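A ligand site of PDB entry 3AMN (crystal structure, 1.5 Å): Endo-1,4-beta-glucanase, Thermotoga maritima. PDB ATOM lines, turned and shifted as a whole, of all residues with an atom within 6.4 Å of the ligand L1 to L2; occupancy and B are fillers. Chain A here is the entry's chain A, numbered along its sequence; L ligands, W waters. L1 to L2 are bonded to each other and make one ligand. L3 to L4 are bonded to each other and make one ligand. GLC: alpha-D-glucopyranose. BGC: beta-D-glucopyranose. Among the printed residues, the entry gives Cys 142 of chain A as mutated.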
ATOM      1  N   GLU A  30      25.107  -4.228  16.742  1.00  0.00           N
ATOM      2  CA  GLU A  30      24.418  -5.410  17.170  1.00  0.00           C
ATOM      3  C   GLU A  30      23.313  -5.764  16.174  1.00  0.00           C
ATOM      4  O   GLU A  30      22.382  -4.971  15.928  1.00  0.00           O
ATOM      5  CB  GLU A  30      23.793  -5.245  18.604  1.00  0.00           C
ATOM      6  CG  GLU A  30      23.297  -6.588  19.139  1.00  0.00           C
ATOM      7  CD  GLU A  30      22.526  -6.546  20.440  1.00  0.00           C
ATOM      8  OE1 GLU A  30      22.755  -5.641  21.248  1.00  0.00           O
ATOM      9  OE2 GLU A  30      21.654  -7.459  20.638  1.00  0.00           O
ATOM     10  N   ASN A  32      20.504  -7.238  16.203  1.00  0.00           N
ATOM     11  CA  ASN A  32      19.699  -7.506  17.380  1.00  0.00           C
ATOM     12  C   ASN A  32      18.296  -7.971  17.066  1.00  0.00           C
ATOM     13  O   ASN A  32      17.445  -7.174  16.661  1.00  0.00           O
ATOM     14  CB  ASN A  32      19.706  -6.188  18.170  1.00  0.00           C
ATOM     15  CG  ASN A  32      18.883  -6.236  19.460  1.00  0.00           C
ATOM     16  OD1 ASN A  32      18.296  -7.297  19.752  1.00  0.00           O
ATOM     17  ND2 ASN A  32      18.843  -5.163  20.226  1.00  0.00           N
ATOM     18  N   TRP A  34      16.307  -9.475  19.368  1.00  0.00           N
ATOM     19  CA  TRP A  34      16.143  -9.908  20.768  1.00  0.00           C
ATOM     20  C   TRP A  34      14.881 -10.579  21.129  1.00  0.00           C
ATOM     21  O   TRP A  34      14.885 -11.424  22.061  1.00  0.00           O
ATOM     22  CB  TRP A  34      16.404  -8.734  21.742  1.00  0.00           C
ATOM     23  CG  TRP A  34      15.425  -7.631  21.713  1.00  0.00           C
ATOM     24  CD1 TRP A  34      15.423  -6.540  20.870  1.00  0.00           C
ATOM     25  CD2 TRP A  34      14.280  -7.488  22.560  1.00  0.00           C
ATOM     26  NE1 TRP A  34      14.324  -5.710  21.180  1.00  0.00           N
ATOM     27  CE2 TRP A  34      13.631  -6.279  22.209  1.00  0.00           C
ATOM     28  CE3 TRP A  34      13.753  -8.271  23.614  1.00  0.00           C
ATOM     29  CZ2 TRP A  34      12.478  -5.835  22.878  1.00  0.00           C
ATOM     30  CZ3 TRP A  34      12.621  -7.802  24.259  1.00  0.00           C
ATOM     31  CH2 TRP A  34      12.022  -6.632  23.896  1.00  0.00           C
ATOM     32  N   ARG A  68       6.175  -8.035  24.893  1.00  0.00           N
ATOM     33  CA  ARG A  68       7.154  -6.993  24.580  1.00  0.00           C
ATOM     34  C   ARG A  68       6.855  -6.294  23.273  1.00  0.00           C
ATOM     35  O   ARG A  68       7.496  -5.264  22.966  1.00  0.00           O
ATOM     36  CB  ARG A  68       8.571  -7.564  24.543  1.00  0.00           C
ATOM     37  CG  ARG A  68       8.972  -8.254  25.842  1.00  0.00           C
ATOM     38  CD  ARG A  68       8.725  -7.461  27.143  1.00  0.00           C
ATOM     39  NE  ARG A  68       9.349  -6.145  27.091  1.00  0.00           N
ATOM     40  CZ  ARG A  68      10.669  -5.956  27.145  1.00  0.00           C
ATOM     41  NH1 ARG A  68      11.466  -7.001  27.277  1.00  0.00           N
ATOM     42  NH2 ARG A  68      11.155  -4.740  27.057  1.00  0.00           N
ATOM     43  N   VAL A  70       7.399  -5.566  20.097  1.00  0.00           N
ATOM     44  CA  VAL A  70       8.347  -5.560  18.976  1.00  0.00           C
ATOM     45  C   VAL A  70       9.164  -6.827  18.897  1.00  0.00           C
ATOM     46  O   VAL A  70       9.220  -7.625  19.857  1.00  0.00           O
ATOM     47  CB  VAL A  70       9.300  -4.365  19.071  1.00  0.00           C
ATOM     48  CG1 VAL A  70       8.474  -3.068  18.978  1.00  0.00           C
ATOM     49  CG2 VAL A  70      10.182  -4.448  20.299  1.00  0.00           C
ATOM     50  N   GLY A  72      12.559  -6.901  17.229  1.00  0.00           N
ATOM     51  CA  GLY A  72      14.015  -6.717  17.267  1.00  0.00           C
ATOM     52  C   GLY A  72      14.367  -5.248  17.145  1.00  0.00           C
ATOM     53  O   GLY A  72      13.485  -4.376  17.003  1.00  0.00           O
ATOM     54  N   TYR A  73      15.687  -4.986  17.184  1.00  0.00           N
ATOM     55  CA  TYR A  73      16.217  -3.609  17.155  1.00  0.00           C
ATOM     56  C   TYR A  73      17.640  -3.600  16.600  1.00  0.00           C
ATOM     57  O   TYR A  73      18.596  -3.270  17.331  1.00  0.00           O
ATOM     58  CB  TYR A  73      16.164  -3.005  18.584  1.00  0.00           C
ATOM     59  CG  TYR A  73      16.645  -1.591  18.729  1.00  0.00           C
ATOM     60  CD1 TYR A  73      16.159  -0.565  17.933  1.00  0.00           C
ATOM     61  CD2 TYR A  73      17.532  -1.252  19.749  1.00  0.00           C
ATOM     62  CE1 TYR A  73      16.525   0.766  18.173  1.00  0.00           C
ATOM     63  CE2 TYR A  73      17.945   0.074  19.965  1.00  0.00           C
ATOM     64  CZ  TYR A  73      17.433   1.087  19.185  1.00  0.00           C
ATOM     65  OH  TYR A  73      17.827   2.402  19.405  1.00  0.00           O
ATOM     66  N   GLU A  75      20.922  -2.281  15.381  1.00  0.00           N
ATOM     67  CA  GLU A  75      21.404  -1.010  15.864  1.00  0.00           C
ATOM     68  C   GLU A  75      22.926  -0.913  15.966  1.00  0.00           C
ATOM     69  O   GLU A  75      23.624  -1.906  15.790  1.00  0.00           O
ATOM     70  CB  GLU A  75      20.881  -0.812  17.335  1.00  0.00           C
ATOM     71  CG  GLU A  75      21.448  -1.950  18.240  1.00  0.00           C
ATOM     72  CD  GLU A  75      21.134  -1.805  19.721  1.00  0.00           C
ATOM     73  OE1 GLU A  75      21.473  -0.755  20.278  1.00  0.00           O
ATOM     74  OE2 GLU A  75      20.584  -2.750  20.338  1.00  0.00           O
ATOM     75  N   LYS A  81      25.928  -0.882  26.923  1.00  0.00           N
ATOM     76  CA  LYS A  81      24.539  -1.342  26.871  1.00  0.00           C
ATOM     77  C   LYS A  81      24.342  -2.276  28.069  1.00  0.00           C
ATOM     78  O   LYS A  81      24.863  -3.412  28.067  1.00  0.00           O
ATOM     79  CB  LYS A  81      24.274  -2.046  25.528  1.00  0.00           C
ATOM     80  CG  LYS A  81      22.865  -2.490  25.410  1.00  0.00           C
ATOM     81  CD  LYS A  81      22.585  -3.078  24.020  1.00  0.00           C
ATOM     82  CE  LYS A  81      21.221  -3.638  24.055  1.00  0.00           C
ATOM     83  NZ  LYS A  81      20.867  -4.225  22.722  1.00  0.00           N
ATOM     84  N   TRP A  83      21.986  -4.351  29.122  1.00  0.00           N
ATOM     85  CA  TRP A  83      21.463  -5.678  28.844  1.00  0.00           C
ATOM     86  C   TRP A  83      22.474  -6.628  28.237  1.00  0.00           C
ATOM     87  O   TRP A  83      22.311  -7.854  28.380  1.00  0.00           O
ATOM     88  CB  TRP A  83      20.282  -5.588  27.892  1.00  0.00           C
ATOM     89  CG  TRP A  83      19.232  -4.725  28.414  1.00  0.00           C
ATOM     90  CD1 TRP A  83      18.955  -3.403  28.067  1.00  0.00           C
ATOM     91  CD2 TRP A  83      18.281  -5.069  29.424  1.00  0.00           C
ATOM     92  NE1 TRP A  83      17.897  -2.931  28.802  1.00  0.00           N
ATOM     93  CE2 TRP A  83      17.465  -3.919  29.648  1.00  0.00           C
ATOM     94  CE3 TRP A  83      18.033  -6.236  30.165  1.00  0.00           C
ATOM     95  CZ2 TRP A  83      16.402  -3.936  30.589  1.00  0.00           C
ATOM     96  CZ3 TRP A  83      16.988  -6.242  31.102  1.00  0.00           C
ATOM     97  CH2 TRP A  83      16.191  -5.104  31.302  1.00  0.00           C
ATOM     98  N   GLU A  84      23.504  -6.136  27.564  1.00  0.00           N
ATOM     99  CA  GLU A  84      24.499  -7.036  26.980  1.00  0.00           C
ATOM    100  C   GLU A  84      25.794  -6.996  27.780  1.00  0.00           C
ATOM    101  O   GLU A  84      26.775  -7.647  27.415  1.00  0.00           O
ATOM    102  CB  GLU A  84      24.746  -6.651  25.496  1.00  0.00           C
ATOM    103  CG  GLU A  84      23.567  -7.027  24.561  1.00  0.00           C
ATOM    104  CD  GLU A  84      23.280  -8.539  24.566  1.00  0.00           C
ATOM    105  OE1 GLU A  84      24.241  -9.308  24.653  1.00  0.00           O
ATOM    106  OE2 GLU A  84      22.097  -8.970  24.502  1.00  0.00           O
ATOM    107  N   GLU A 124      18.138   5.616  21.640  1.00  0.00           N
ATOM    108  CA  GLU A 124      17.802   5.485  23.025  1.00  0.00           C
ATOM    109  C   GLU A 124      18.950   5.427  23.972  1.00  0.00           C
ATOM    110  O   GLU A 124      20.091   5.112  23.594  1.00  0.00           O
ATOM    111  CB  GLU A 124      16.886   4.293  23.309  1.00  0.00           C
ATOM    112  CG  GLU A 124      17.502   3.002  23.213  1.00  0.00           C
ATOM    113  CD  GLU A 124      16.581   1.825  23.685  1.00  0.00           C
ATOM    114  OE1 GLU A 124      17.090   0.705  23.793  1.00  0.00           O
ATOM    115  OE2 GLU A 124      15.350   1.955  23.887  1.00  0.00           O
ATOM    116  N   TRP A 126      19.781   4.326  28.370  1.00  0.00           N
ATOM    117  CA  TRP A 126      19.354   3.694  29.601  1.00  0.00           C
ATOM    118  C   TRP A 126      20.013   4.485  30.761  1.00  0.00           C
ATOM    119  O   TRP A 126      21.233   4.666  30.797  1.00  0.00           O
ATOM    120  CB  TRP A 126      19.778   2.213  29.671  1.00  0.00           C
ATOM    121  CG  TRP A 126      19.107   1.391  28.630  1.00  0.00           C
ATOM    122  CD1 TRP A 126      19.541   1.193  27.363  1.00  0.00           C
ATOM    123  CD2 TRP A 126      17.844   0.768  28.721  1.00  0.00           C
ATOM    124  NE1 TRP A 126      18.618   0.460  26.637  1.00  0.00           N
ATOM    125  CE2 TRP A 126      17.570   0.209  27.461  1.00  0.00           C
ATOM    126  CE3 TRP A 126      16.912   0.619  29.747  1.00  0.00           C
ATOM    127  CZ2 TRP A 126      16.377  -0.515  27.191  1.00  0.00           C
ATOM    128  CZ3 TRP A 126      15.728  -0.113  29.498  1.00  0.00           C
ATOM    129  CH2 TRP A 126      15.488  -0.662  28.225  1.00  0.00           C
ATOM    130  N   CYS A 142      14.401   4.383  30.744  1.00  0.00           N
ATOM    131  CA  CYS A 142      14.781   4.262  29.361  1.00  0.00           C
ATOM    132  C   CYS A 142      14.257   5.497  28.633  1.00  0.00           C
ATOM    133  O   CYS A 142      13.058   5.831  28.835  1.00  0.00           O
ATOM    134  CB  CYS A 142      14.168   3.026  28.762  1.00  0.00           C
ATOM    135  SG  CYS A 142      14.429   2.929  26.948  1.00  0.00           S
ATOM    136  N   MET A 144      13.740   7.124  24.795  1.00  0.00           N
ATOM    137  CA  MET A 144      13.883   6.931  23.358  1.00  0.00           C
ATOM    138  C   MET A 144      13.548   8.226  22.631  1.00  0.00           C
ATOM    139  O   MET A 144      12.770   9.049  23.144  1.00  0.00           O
ATOM    140  CB  MET A 144      12.926   5.865  22.823  1.00  0.00           C
ATOM    141  CG  MET A 144      13.003   4.541  23.574  1.00  0.00           C
ATOM    142  SD  MET A 144      12.073   3.276  22.688  1.00  0.00           S
ATOM    143  CE  MET A 144      13.283   2.790  21.537  1.00  0.00           C
ATOM    144  N   TRP A 184       6.800   0.328  33.585  1.00  0.00           N
ATOM    145  CA  TRP A 184       6.887  -1.096  33.477  1.00  0.00           C
ATOM    146  C   TRP A 184       7.839  -1.560  34.554  1.00  0.00           C
ATOM    147  O   TRP A 184       7.746  -1.085  35.679  1.00  0.00           O
ATOM    148  CB  TRP A 184       7.400  -1.491  32.091  1.00  0.00           C
ATOM    149  CG  TRP A 184       6.433  -1.166  30.935  1.00  0.00           C
ATOM    150  CD1 TRP A 184       5.077  -1.221  30.940  1.00  0.00           C
ATOM    151  CD2 TRP A 184       6.811  -0.796  29.603  1.00  0.00           C
ATOM    152  NE1 TRP A 184       4.569  -0.891  29.697  1.00  0.00           N
ATOM    153  CE2 TRP A 184       5.623  -0.637  28.861  1.00  0.00           C
ATOM    154  CE3 TRP A 184       8.048  -0.576  28.969  1.00  0.00           C
ATOM    155  CZ2 TRP A 184       5.623  -0.267  27.506  1.00  0.00           C
ATOM    156  CZ3 TRP A 184       8.047  -0.206  27.638  1.00  0.00           C
ATOM    157  CH2 TRP A 184       6.832  -0.055  26.921  1.00  0.00           C
ATOM    158  N   TRP A 186      10.738  -0.736  34.604  1.00  0.00           N
ATOM    159  CA  TRP A 186      11.530   0.498  34.722  1.00  0.00           C
ATOM    160  C   TRP A 186      10.622   1.563  34.066  1.00  0.00           C
ATOM    161  O   TRP A 186       9.528   1.200  33.589  1.00  0.00           O
ATOM    162  CB  TRP A 186      12.871   0.391  33.957  1.00  0.00           C
ATOM    163  CG  TRP A 186      12.667  -0.083  32.528  1.00  0.00           C
ATOM    164  CD1 TRP A 186      12.449   0.731  31.407  1.00  0.00           C
ATOM    165  CD2 TRP A 186      12.706  -1.429  32.029  1.00  0.00           C
ATOM    166  NE1 TRP A 186      12.360  -0.057  30.288  1.00  0.00           N
ATOM    167  CE2 TRP A 186      12.509  -1.372  30.639  1.00  0.00           C
ATOM    168  CE3 TRP A 186      12.901  -2.681  32.645  1.00  0.00           C
ATOM    169  CZ2 TRP A 186      12.507  -2.544  29.834  1.00  0.00           C
ATOM    170  CZ3 TRP A 186      12.897  -3.847  31.848  1.00  0.00           C
ATOM    171  CH2 TRP A 186      12.708  -3.769  30.457  1.00  0.00           C
ATOM    172  N   TYR A 188       9.658   4.024  31.106  1.00  0.00           N
ATOM    173  CA  TYR A 188       9.890   4.181  29.666  1.00  0.00           C
ATOM    174  C   TYR A 188       9.366   5.532  29.219  1.00  0.00           C
ATOM    175  O   TYR A 188       8.191   5.881  29.478  1.00  0.00           O
ATOM    176  CB  TYR A 188       9.123   3.076  28.978  1.00  0.00           C
ATOM    177  CG  TYR A 188       8.955   3.207  27.492  1.00  0.00           C
ATOM    178  CD1 TYR A 188       9.838   2.561  26.641  1.00  0.00           C
ATOM    179  CD2 TYR A 188       7.848   3.875  26.932  1.00  0.00           C
ATOM    180  CE1 TYR A 188       9.617   2.531  25.231  1.00  0.00           C
ATOM    181  CE2 TYR A 188       7.618   3.873  25.538  1.00  0.00           C
ATOM    182  CZ  TYR A 188       8.510   3.176  24.701  1.00  0.00           C
ATOM    183  OH  TYR A 188       8.265   3.176  23.339  1.00  0.00           O
ATOM    184  N   GLU A 235      22.187   4.506  21.709  1.00  0.00           N
ATOM    185  CA  GLU A 235      21.890   3.490  20.715  1.00  0.00           C
ATOM    186  C   GLU A 235      21.126   4.086  19.575  1.00  0.00           C
ATOM    187  O   GLU A 235      20.286   4.986  19.796  1.00  0.00           O
ATOM    188  CB  GLU A 235      21.024   2.394  21.329  1.00  0.00           C
ATOM    189  CG  GLU A 235      21.661   1.686  22.544  1.00  0.00           C
ATOM    190  CD  GLU A 235      20.775   0.632  23.136  1.00  0.00           C
ATOM    191  OE1 GLU A 235      20.525  -0.486  22.585  1.00  0.00           O
ATOM    192  OE2 GLU A 235      20.281   0.875  24.246  1.00  0.00           O
ATOM    193  N   GLU A 239      13.553  -0.273  15.608  1.00  0.00           N
ATOM    194  CA  GLU A 239      12.719  -1.372  16.132  1.00  0.00           C
ATOM    195  C   GLU A 239      11.775  -1.834  15.061  1.00  0.00           C
ATOM    196  O   GLU A 239      11.368  -1.032  14.193  1.00  0.00           O
ATOM    197  CB  GLU A 239      11.852  -0.915  17.305  1.00  0.00           C
ATOM    198  CG  GLU A 239      12.619  -0.435  18.509  1.00  0.00           C
ATOM    199  CD  GLU A 239      11.697  -0.201  19.690  1.00  0.00           C
ATOM    200  OE1 GLU A 239      11.060   0.901  19.802  1.00  0.00           O
ATOM    201  OE2 GLU A 239      11.568  -1.115  20.529  1.00  0.00           O
HETATM  202  C1  GLC L   1      12.371  -0.375  24.120  1.00  0.00           C
HETATM  203  C2  GLC L   1      12.159  -1.606  25.002  1.00  0.00           C
HETATM  204  C3  GLC L   1      13.527  -2.165  25.382  1.00  0.00           C
HETATM  205  C4  GLC L   1      14.216  -2.669  24.102  1.00  0.00           C
HETATM  206  C5  GLC L   1      14.263  -1.524  23.107  1.00  0.00           C
HETATM  207  C6  GLC L   1      14.646  -2.021  21.715  1.00  0.00           C
HETATM  208  O1  GLC L   1      13.218   0.573  24.764  1.00  0.00           O
HETATM  209  O2  GLC L   1      11.438  -1.211  26.165  1.00  0.00           O
HETATM  210  O3  GLC L   1      13.379  -3.228  26.334  1.00  0.00           O
HETATM  211  O4  GLC L   1      15.602  -2.958  24.370  1.00  0.00           O
HETATM  212  O5  GLC L   1      13.029  -0.828  22.921  1.00  0.00           O
HETATM  213  O6  GLC L   1      13.626  -2.871  21.187  1.00  0.00           O
HETATM  214  C2  BGC L   2      17.400  -4.532  24.144  1.00  0.00           C
HETATM  215  C3  BGC L   2      17.715  -6.017  24.266  1.00  0.00           C
HETATM  216  C4  BGC L   2      17.324  -6.487  25.666  1.00  0.00           C
HETATM  217  C5  BGC L   2      15.862  -6.144  25.952  1.00  0.00           C
HETATM  218  C6  BGC L   2      15.532  -6.478  27.407  1.00  0.00           C
HETATM  219  C1  BGC L   2      15.917  -4.354  24.417  1.00  0.00           C
HETATM  220  O2  BGC L   2      17.721  -4.076  22.826  1.00  0.00           O
HETATM  221  O3  BGC L   2      19.120  -6.206  24.095  1.00  0.00           O
HETATM  222  O4  BGC L   2      17.456  -7.912  25.705  1.00  0.00           O
HETATM  223  O5  BGC L   2      15.659  -4.752  25.771  1.00  0.00           O
HETATM  224  O6  BGC L   2      14.183  -6.141  27.722  1.00  0.00           O
HETATM  225  C2  BGC L   3       1.933  -2.124  23.662  1.00  0.00           C
HETATM  226  C3  BGC L   3       3.310  -1.463  23.633  1.00  0.00           C
HETATM  227  C4  BGC L   3       3.731  -1.227  22.181  1.00  0.00           C
HETATM  228  C5  BGC L   3       2.627  -0.545  21.388  1.00  0.00           C
HETATM  229  C6  BGC L   3       2.969  -0.499  19.903  1.00  0.00           C
HETATM  230  C1  BGC L   3       0.944  -1.246  22.907  1.00  0.00           C
HETATM  231  O1  BGC L   3      -0.372  -1.796  22.972  1.00  0.00           O
HETATM  232  O2  BGC L   3       1.518  -2.263  25.035  1.00  0.00           O
HETATM  233  O3  BGC L   3       4.261  -2.295  24.309  1.00  0.00           O
HETATM  234  O4  BGC L   3       4.796  -0.266  22.180  1.00  0.00           O
HETATM  235  O5  BGC L   3       1.346  -1.179  21.532  1.00  0.00           O
HETATM  236  O6  BGC L   3       2.027   0.304  19.186  1.00  0.00           O
HETATM  237  C2  BGC L   4       6.997   0.420  21.747  1.00  0.00           C
HETATM  238  C3  BGC L   4       8.479   0.060  21.739  1.00  0.00           C
HETATM  239  C4  BGC L   4       8.822  -0.797  22.955  1.00  0.00           C
HETATM  240  C5  BGC L   4       7.821  -1.933  23.169  1.00  0.00           C
HETATM  241  C6  BGC L   4       8.201  -2.791  24.381  1.00  0.00           C
HETATM  242  C1  BGC L   4       6.119  -0.801  22.073  1.00  0.00           C
HETATM  243  O2  BGC L   4       6.637   0.937  20.468  1.00  0.00           O
HETATM  244  O3  BGC L   4       9.304   1.236  21.769  1.00  0.00           O
HETATM  245  O4  BGC L   4      10.080  -1.430  22.691  1.00  0.00           O
HETATM  246  O5  BGC L   4       6.534  -1.325  23.332  1.00  0.00           O
HETATM  247  O6  BGC L   4       9.294  -3.671  24.067  1.00  0.00           O
HETATM  248  O   HOH W   1      20.225  -8.163  22.714  1.00  0.00           O
HETATM  249  O   HOH W   2      15.824  -9.995  26.554  1.00  0.00           O
HETATM  250  O   HOH W   3      13.508  -7.548  30.115  1.00  0.00           O
HETATM  251  O   HOH W   4      19.842  -8.839  26.412  1.00  0.00           O
HETATM  252  O   HOH W   5      18.256  -1.605  23.370  1.00  0.00           O
HETATM  253  O   HOH W   6      12.385   0.624  27.575  1.00  0.00           O
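The side-chain hydroxyl of Tyr 188 is in hydrogen-bond range of an oxygen (O3) of BGC L4 (2.7 Å).
ND2 of Asn 32 sits at hydrogen-bond distance from O2 of BGC L2, 3.0 Å away.
SD of Met 144 is in hydrogen-bond range of O3 of BGC L4 (3.6 Å).
SD of Met 144 lies within hydrogen-bond range of O1 of GLC L1, 3.6 Å away.
OE2 of Glu 239 lies within hydrogen-bond range of O6 of GLC L1, 2.8 Å away.
O of Arg 68 sits at hydrogen-bond distance from O6 of BGC L4, 2.6 Å away.
NZ of Lys 81 is in hydrogen-bond range of O3 of BGC L2, 3.0 Å away.
An oxygen (O1) of GLC L1 sits at hydrogen-bond distance from the side-chain carboxylate of Glu 124, 2.7 Å away.
NE1 of Trp 34 sits at hydrogen-bond distance from O6 of GLC L1.
NH2 of Arg 68 sits at hydrogen-bond distance from O3 of GLC L1, at 2.8 Å.
An oxygen (O1) of GLC L1 lies within hydrogen-bond range of the side-chain sulfur (SG) of Cys 142.
An oxygen (O4) of BGC L4 lies within hydrogen-bond range of the side-chain carboxylate of Glu 239 (2.6 Å).
Water W6 lies within hydrogen-bond range of O2 of GLC L1, NE1 of Trp 186 and SG of Cys 142.
Water W5 lies within hydrogen-bond range of O2 of BGC L2 (2.6 Å), OE1 of Glu 124 (2.6 Å) and OE1 of Glu 235 (2.6 Å).
Water W1 lies within hydrogen-bond range of the side-chain carboxylate (OE2) of Glu 30, an oxygen (O3) of BGC L2 and the side-chain carboxylate (OE2) of Glu 84.
Water W4 lies within hydrogen-bond range of an oxygen (O4) of BGC L2, the side-chain carboxylate (OE2) of Glu 84 and the backbone carbonyl oxygen (O) of Trp 83.
The side-chain amide nitrogen (ND2) of Asn 32 sits close to the side-chain amino group (NZ) of Lys 81, 3.3 Å away.
The side-chain carboxylate (OE1) of Glu 30 lies within salt-bridge range of the side-chain amino group (NZ) of Lys 81, at 2.8 Å.
ND2 of Asn 32 sits at hydrogen-bond distance from OE2 of Glu 75 (3.0 Å).
The indole nitrogen (NE1) of Trp 126 lies within hydrogen-bond range of the side-chain carboxylate (OE2) of Glu 235.
The side-chain amide oxygen of Asn 32 lies close to the side-chain carboxylate of Glu 30 (3.5 Å).
OE2 of Glu 75 is in salt-bridge range of NZ of Lys 81 (2.8 Å).
The side-chain amino group (NZ) of Lys 81 is in salt-bridge range of the side-chain carboxylate (OE1) of Glu 235, 3.8 Å away.
OE2 of Glu 124 lies within hydrogen-bond range of SG of Cys 142 (3.3 Å).
An oxygen (O5) of GLC L1 sits close to an oxygen (O4) of BGC L4 (3.0 Å).
Residues that only touch the ligand L1 to L2: Tyr 73 (3.6 Å), Trp 186 (3.7 Å), Trp 83 (3.7 Å), Trp 126 (3.8 Å), Trp 184 (3.8 Å) and Val 70 (3.9 Å).
Hydrophobic or aromatic side chains that line the ligand L1 to L2: Trp 34, Val 70, Tyr 73, Trp 83, Trp 126, Met 144, Trp 184 and Trp 186.
Within 4 Å of the ligand L1 to L2: Asn 32, Trp 34, Arg 68, Val 70, Tyr 73, Lys 81, Trp 83, Glu 124, Trp 126, Cys 142, Met 144, Trp 184, Trp 186 and Glu 239.
The nearest printed residue that does not touch the ligand L1 to L2 is Glu 75 (4.02 Å).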
